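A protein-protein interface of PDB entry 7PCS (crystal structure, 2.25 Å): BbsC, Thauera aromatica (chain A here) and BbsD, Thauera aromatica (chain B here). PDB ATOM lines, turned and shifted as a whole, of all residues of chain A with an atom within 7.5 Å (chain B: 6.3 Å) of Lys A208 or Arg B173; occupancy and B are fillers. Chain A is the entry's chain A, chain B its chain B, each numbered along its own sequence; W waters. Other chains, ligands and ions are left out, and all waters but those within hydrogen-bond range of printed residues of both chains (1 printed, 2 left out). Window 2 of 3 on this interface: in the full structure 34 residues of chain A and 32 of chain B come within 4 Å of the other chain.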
ATOM      1  N   ARG A 198     -33.535  11.816  -1.871  1.00  0.00           N
ATOM      2  CA  ARG A 198     -32.155  11.525  -2.234  1.00  0.00           C
ATOM      3  C   ARG A 198     -31.319  11.339  -0.976  1.00  0.00           C
ATOM      4  O   ARG A 198     -30.544  10.383  -0.863  1.00  0.00           O
ATOM      5  CB  ARG A 198     -31.543  12.654  -3.065  1.00  0.00           C
ATOM      6  CG  ARG A 198     -32.252  13.031  -4.356  1.00  0.00           C
ATOM      7  CD  ARG A 198     -31.308  13.853  -5.224  1.00  0.00           C
ATOM      8  NE  ARG A 198     -31.959  14.355  -6.424  1.00  0.00           N
ATOM      9  CZ  ARG A 198     -32.397  15.600  -6.532  1.00  0.00           C
ATOM     10  NH1 ARG A 198     -32.138  16.501  -5.599  1.00  0.00           N
ATOM     11  NH2 ARG A 198     -33.085  15.957  -7.610  1.00  0.00           N
ATOM     12  N   GLU A 199     -31.468  12.263  -0.016  1.00  0.00           N
ATOM     13  CA  GLU A 199     -30.698  12.179   1.222  1.00  0.00           C
ATOM     14  C   GLU A 199     -31.020  10.900   1.971  1.00  0.00           C
ATOM     15  O   GLU A 199     -30.132  10.277   2.561  1.00  0.00           O
ATOM     16  CB  GLU A 199     -30.962  13.395   2.114  1.00  0.00           C
ATOM     17  CG  GLU A 199     -32.422  13.634   2.521  1.00  0.00           C
ATOM     18  CD  GLU A 199     -32.605  14.939   3.292  1.00  0.00           C
ATOM     19  OE1 GLU A 199     -31.596  15.553   3.703  1.00  0.00           O
ATOM     20  OE2 GLU A 199     -33.767  15.324   3.534  1.00  0.00           O
ATOM     21  N   LEU A 201     -32.239   8.024   0.536  1.00  0.00           N
ATOM     22  CA  LEU A 201     -31.780   6.874  -0.239  1.00  0.00           C
ATOM     23  C   LEU A 201     -30.264   6.725  -0.183  1.00  0.00           C
ATOM     24  O   LEU A 201     -29.753   5.608  -0.044  1.00  0.00           O
ATOM     25  CB  LEU A 201     -32.251   7.007  -1.685  1.00  0.00           C
ATOM     26  CG  LEU A 201     -33.679   6.565  -1.991  1.00  0.00           C
ATOM     27  CD1 LEU A 201     -34.094   6.976  -3.392  1.00  0.00           C
ATOM     28  CD2 LEU A 201     -33.796   5.051  -1.840  1.00  0.00           C
ATOM     29  N   ALA A 202     -29.528   7.833  -0.295  1.00  0.00           N
ATOM     30  CA  ALA A 202     -28.071   7.744  -0.338  1.00  0.00           C
ATOM     31  C   ALA A 202     -27.516   7.117   0.934  1.00  0.00           C
ATOM     32  O   ALA A 202     -26.522   6.383   0.892  1.00  0.00           O
ATOM     33  CB  ALA A 202     -27.466   9.132  -0.558  1.00  0.00           C
ATOM     34  N   GLY A 203     -28.146   7.392   2.075  1.00  0.00           N
ATOM     35  CA  GLY A 203     -27.666   6.832   3.326  1.00  0.00           C
ATOM     36  C   GLY A 203     -27.668   5.321   3.339  1.00  0.00           C
ATOM     37  O   GLY A 203     -26.812   4.702   3.976  1.00  0.00           O
ATOM     38  N   GLY A 204     -28.613   4.709   2.638  1.00  0.00           N
ATOM     39  CA  GLY A 204     -28.731   3.271   2.572  1.00  0.00           C
ATOM     40  C   GLY A 204     -27.882   2.607   1.514  1.00  0.00           C
ATOM     41  O   GLY A 204     -28.030   1.402   1.283  1.00  0.00           O
ATOM     42  N   ILE A 205     -26.992   3.345   0.872  1.00  0.00           N
ATOM     43  CA  ILE A 205     -26.134   2.827  -0.188  1.00  0.00           C
ATOM     44  C   ILE A 205     -24.697   2.877   0.312  1.00  0.00           C
ATOM     45  O   ILE A 205     -24.252   3.936   0.768  1.00  0.00           O
ATOM     46  CB  ILE A 205     -26.288   3.633  -1.490  1.00  0.00           C
ATOM     47  CG1 ILE A 205     -27.758   3.636  -1.926  1.00  0.00           C
ATOM     48  CG2 ILE A 205     -25.405   3.062  -2.570  1.00  0.00           C
ATOM     49  CD1 ILE A 205     -28.045   4.457  -3.167  1.00  0.00           C
ATOM     50  N   PRO A 206     -23.951   1.771   0.256  1.00  0.00           N
ATOM     51  CA  PRO A 206     -22.591   1.780   0.833  1.00  0.00           C
ATOM     52  C   PRO A 206     -21.697   2.902   0.335  1.00  0.00           C
ATOM     53  O   PRO A 206     -20.953   3.477   1.140  1.00  0.00           O
ATOM     54  CB  PRO A 206     -22.040   0.405   0.439  1.00  0.00           C
ATOM     55  CG  PRO A 206     -23.271  -0.490   0.443  1.00  0.00           C
ATOM     56  CD  PRO A 206     -24.394   0.410  -0.111  1.00  0.00           C
ATOM     57  N   VAL A 207     -21.730   3.232  -0.962  1.00  0.00           N
ATOM     58  CA  VAL A 207     -20.894   4.326  -1.453  1.00  0.00           C
ATOM     59  C   VAL A 207     -21.479   5.691  -1.138  1.00  0.00           C
ATOM     60  O   VAL A 207     -20.849   6.708  -1.452  1.00  0.00           O
ATOM     61  CB  VAL A 207     -20.648   4.199  -2.969  1.00  0.00           C
ATOM     62  CG1 VAL A 207     -19.931   2.897  -3.276  1.00  0.00           C
ATOM     63  CG2 VAL A 207     -21.951   4.305  -3.732  1.00  0.00           C
ATOM     64  N   LYS A 208     -22.657   5.745  -0.515  1.00  0.00           N
ATOM     65  CA  LYS A 208     -23.224   6.970   0.051  1.00  0.00           C
ATOM     66  C   LYS A 208     -23.552   8.017  -1.010  1.00  0.00           C
ATOM     67  O   LYS A 208     -23.529   9.215  -0.726  1.00  0.00           O
ATOM     68  CB  LYS A 208     -22.285   7.571   1.100  1.00  0.00           C
ATOM     69  CG  LYS A 208     -21.996   6.633   2.270  1.00  0.00           C
ATOM     70  CD  LYS A 208     -23.266   6.220   2.993  1.00  0.00           C
ATOM     71  CE  LYS A 208     -22.988   5.053   3.954  1.00  0.00           C
ATOM     72  NZ  LYS A 208     -24.122   4.809   4.884  1.00  0.00           N
ATOM     73  N   ARG A 209     -23.837   7.580  -2.235  1.00  0.00           N
ATOM     74  CA  ARG A 209     -24.329   8.466  -3.277  1.00  0.00           C
ATOM     75  C   ARG A 209     -25.357   7.711  -4.103  1.00  0.00           C
ATOM     76  O   ARG A 209     -25.389   6.478  -4.122  1.00  0.00           O
ATOM     77  CB  ARG A 209     -23.197   8.993  -4.176  1.00  0.00           C
ATOM     78  CG  ARG A 209     -22.687   8.030  -5.244  1.00  0.00           C
ATOM     79  CD  ARG A 209     -21.647   8.728  -6.127  1.00  0.00           C
ATOM     80  NE  ARG A 209     -21.054   7.861  -7.142  1.00  0.00           N
ATOM     81  CZ  ARG A 209     -21.596   7.618  -8.331  1.00  0.00           C
ATOM     82  NH1 ARG A 209     -22.801   8.062  -8.647  1.00  0.00           N
ATOM     83  NH2 ARG A 209     -20.912   6.911  -9.227  1.00  0.00           N
ATOM     84  N   LEU A 210     -26.219   8.465  -4.773  1.00  0.00           N
ATOM     85  CA  LEU A 210     -27.140   7.857  -5.716  1.00  0.00           C
ATOM     86  C   LEU A 210     -26.401   7.555  -7.009  1.00  0.00           C
ATOM     87  O   LEU A 210     -25.386   8.178  -7.324  1.00  0.00           O
ATOM     88  CB  LEU A 210     -28.323   8.781  -5.997  1.00  0.00           C
ATOM     89  CG  LEU A 210     -29.320   8.999  -4.864  1.00  0.00           C
ATOM     90  CD1 LEU A 210     -30.338  10.054  -5.288  1.00  0.00           C
ATOM     91  CD2 LEU A 210     -30.011   7.708  -4.489  1.00  0.00           C
ATOM     92  N   GLY A 240     -24.082   0.759  -6.267  1.00  0.00           N
ATOM     93  CA  GLY A 240     -23.371   1.355  -5.159  1.00  0.00           C
ATOM     94  C   GLY A 240     -23.154   0.439  -3.978  1.00  0.00           C
ATOM     95  O   GLY A 240     -22.763   0.913  -2.905  1.00  0.00           O
ATOM     96  N   TYR A 245     -26.844  -6.410   0.149  1.00  0.00           N
ATOM     97  CA  TYR A 245     -27.785  -6.649   1.237  1.00  0.00           C
ATOM     98  C   TYR A 245     -28.825  -7.717   0.903  1.00  0.00           C
ATOM     99  O   TYR A 245     -29.581  -8.123   1.793  1.00  0.00           O
ATOM    100  CB  TYR A 245     -28.504  -5.343   1.596  1.00  0.00           C
ATOM    101  CG  TYR A 245     -27.604  -4.272   2.170  1.00  0.00           C
ATOM    102  CD1 TYR A 245     -26.566  -4.600   3.043  1.00  0.00           C
ATOM    103  CD2 TYR A 245     -27.793  -2.934   1.845  1.00  0.00           C
ATOM    104  CE1 TYR A 245     -25.738  -3.627   3.579  1.00  0.00           C
ATOM    105  CE2 TYR A 245     -26.971  -1.949   2.371  1.00  0.00           C
ATOM    106  CZ  TYR A 245     -25.943  -2.300   3.241  1.00  0.00           C
ATOM    107  OH  TYR A 245     -25.122  -1.326   3.772  1.00  0.00           O
ATOM    108  N   ALA B 168     -17.008  -4.463   0.398  1.00  0.00           N
ATOM    109  CA  ALA B 168     -17.751  -3.535  -0.445  1.00  0.00           C
ATOM    110  C   ALA B 168     -18.698  -2.693   0.397  1.00  0.00           C
ATOM    111  O   ALA B 168     -18.828  -1.479   0.189  1.00  0.00           O
ATOM    112  CB  ALA B 168     -18.528  -4.297  -1.521  1.00  0.00           C
ATOM    113  N   ILE B 169     -19.366  -3.327   1.360  1.00  0.00           N
ATOM    114  CA  ILE B 169     -20.280  -2.602   2.232  1.00  0.00           C
ATOM    115  C   ILE B 169     -19.511  -1.638   3.117  1.00  0.00           C
ATOM    116  O   ILE B 169     -19.904  -0.477   3.283  1.00  0.00           O
ATOM    117  CB  ILE B 169     -21.097  -3.592   3.078  1.00  0.00           C
ATOM    118  CG1 ILE B 169     -21.916  -4.509   2.169  1.00  0.00           C
ATOM    119  CG2 ILE B 169     -22.005  -2.843   4.036  1.00  0.00           C
ATOM    120  CD1 ILE B 169     -22.575  -5.676   2.915  1.00  0.00           C
ATOM    121  N   GLU B 170     -18.403  -2.102   3.694  1.00  0.00           N
ATOM    122  CA  GLU B 170     -17.696  -1.329   4.707  1.00  0.00           C
ATOM    123  C   GLU B 170     -16.900  -0.180   4.101  1.00  0.00           C
ATOM    124  O   GLU B 170     -16.914   0.932   4.638  1.00  0.00           O
ATOM    125  CB  GLU B 170     -16.767  -2.248   5.503  1.00  0.00           C
ATOM    126  CG  GLU B 170     -15.962  -1.537   6.601  1.00  0.00           C
ATOM    127  CD  GLU B 170     -15.043  -2.486   7.355  1.00  0.00           C
ATOM    128  OE1 GLU B 170     -15.462  -3.629   7.637  1.00  0.00           O
ATOM    129  OE2 GLU B 170     -13.900  -2.106   7.673  1.00  0.00           O
ATOM    130  N   LEU B 171     -16.189  -0.428   3.005  1.00  0.00           N
ATOM    131  CA  LEU B 171     -15.257   0.550   2.460  1.00  0.00           C
ATOM    132  C   LEU B 171     -15.896   1.505   1.462  1.00  0.00           C
ATOM    133  O   LEU B 171     -15.234   2.459   1.034  1.00  0.00           O
ATOM    134  CB  LEU B 171     -14.086  -0.172   1.787  1.00  0.00           C
ATOM    135  CG  LEU B 171     -13.386  -1.248   2.614  1.00  0.00           C
ATOM    136  CD1 LEU B 171     -12.189  -1.838   1.888  1.00  0.00           C
ATOM    137  CD2 LEU B 171     -12.953  -0.665   3.959  1.00  0.00           C
ATOM    138  N   GLY B 172     -17.162   1.286   1.094  1.00  0.00           N
ATOM    139  CA  GLY B 172     -17.772   2.100   0.057  1.00  0.00           C
ATOM    140  C   GLY B 172     -17.789   3.575   0.404  1.00  0.00           C
ATOM    141  O   GLY B 172     -17.581   4.430  -0.462  1.00  0.00           O
ATOM    142  N   ARG B 173     -18.035   3.894   1.676  1.00  0.00           N
ATOM    143  CA  ARG B 173     -18.117   5.289   2.078  1.00  0.00           C
ATOM    144  C   ARG B 173     -16.791   6.018   1.912  1.00  0.00           C
ATOM    145  O   ARG B 173     -16.783   7.248   1.812  1.00  0.00           O
ATOM    146  CB  ARG B 173     -18.624   5.387   3.520  1.00  0.00           C
ATOM    147  CG  ARG B 173     -17.858   4.589   4.561  1.00  0.00           C
ATOM    148  CD  ARG B 173     -18.797   4.154   5.722  1.00  0.00           C
ATOM    149  NE  ARG B 173     -19.875   3.239   5.345  1.00  0.00           N
ATOM    150  CZ  ARG B 173     -21.007   3.090   6.026  1.00  0.00           C
ATOM    151  NH1 ARG B 173     -21.246   3.776   7.135  1.00  0.00           N
ATOM    152  NH2 ARG B 173     -21.919   2.223   5.592  1.00  0.00           N
ATOM    153  N   ALA B 174     -15.677   5.297   1.851  1.00  0.00           N
ATOM    154  CA  ALA B 174     -14.372   5.912   1.676  1.00  0.00           C
ATOM    155  C   ALA B 174     -13.974   6.046   0.214  1.00  0.00           C
ATOM    156  O   ALA B 174     -12.824   6.402  -0.069  1.00  0.00           O
ATOM    157  CB  ALA B 174     -13.309   5.109   2.424  1.00  0.00           C
ATOM    158  N   GLY B 175     -14.892   5.782  -0.712  1.00  0.00           N
ATOM    159  CA  GLY B 175     -14.565   5.847  -2.123  1.00  0.00           C
ATOM    160  C   GLY B 175     -13.864   4.622  -2.660  1.00  0.00           C
ATOM    161  O   GLY B 175     -13.204   4.704  -3.704  1.00  0.00           O
ATOM    162  N   ILE B 176     -13.988   3.488  -1.976  1.00  0.00           N
ATOM    163  CA  ILE B 176     -13.348   2.240  -2.369  1.00  0.00           C
ATOM    164  C   ILE B 176     -14.428   1.275  -2.843  1.00  0.00           C
ATOM    165  O   ILE B 176     -15.417   1.037  -2.136  1.00  0.00           O
ATOM    166  CB  ILE B 176     -12.543   1.640  -1.202  1.00  0.00           C
ATOM    167  CG1 ILE B 176     -11.481   2.634  -0.721  1.00  0.00           C
ATOM    168  CG2 ILE B 176     -11.903   0.332  -1.621  1.00  0.00           C
ATOM    169  CD1 ILE B 176     -10.729   2.189   0.510  1.00  0.00           C
HETATM  170  O   HOH W   1     -24.149   2.237   4.368  1.00  0.00           O
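Of the printed residues of chain B, Val A207 touches Gly B172. Of chain B, only Arg B173 (3.4 Å) comes within 4 Å of Lys A208. Of the printed residues of chain A, Ala B168 touches Pro A206. Glu B170 touches none of the printed residues of chain A. Of chain A, only Pro A206 and Lys A208 come within 4 Å of Arg B173. The nearest residue of chain B that does not touch Lys A208 is Gly B172 (5.2 Å). The nearest printed residue of chain A that does not touch Ala B168 is Gly A240 (5.5 Å).
The backbone NH (N) of Arg B173 is in hydrogen-bond range of the backbone carbonyl oxygen (O) of Pro A206 (3.0 Å). The side-chain amino group of Lys A208 sits close to the guanidinium group of Arg B173, 3.5 Å away.
Water W1 bridges the guanidinium group of Arg B173 and the side-chain amino group of Lys A208.
The backbone NH (N) of Val A207 sits at hydrogen-bond distance from the backbone carbonyl oxygen (O) of Gly A240, at 3.2 Å. The side-chain amino group of Lys A208 sits at hydrogen-bond distance from the backbone carbonyl oxygen of Gly A203.
Among the printed residues, merely in contact across the chains: Pro A206 with Gly B172 (3.2 Å), Val A207 with Gly B172 (3.5 Å), Tyr A245 with Ile B169 (3.5 Å), Pro A206 with Ile B169 (3.7 Å) and Pro A206 with Ala B168 (3.7 Å).
Printed residues of chain B that touch a printed residue of chain A: Ala B168, Ile B169, Gly B172 and Arg B173. Hydrophobic or aromatic side chains of chain B within 4 Å of the printed part of chain A: Ile B169. Of the 14 printed residues of chain A, 4 touch a printed residue of chain B. Printed residues of chain A that touch a printed residue of chain B: Pro A206, Val A207, Lys A208 and Tyr A245. Among the printed residues, 7 pairs touch across the chains. Among the printed residues, no Asp or Glu carboxylate lies within 4 Å of a Lys or Arg side-chain nitrogen of the other chain.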
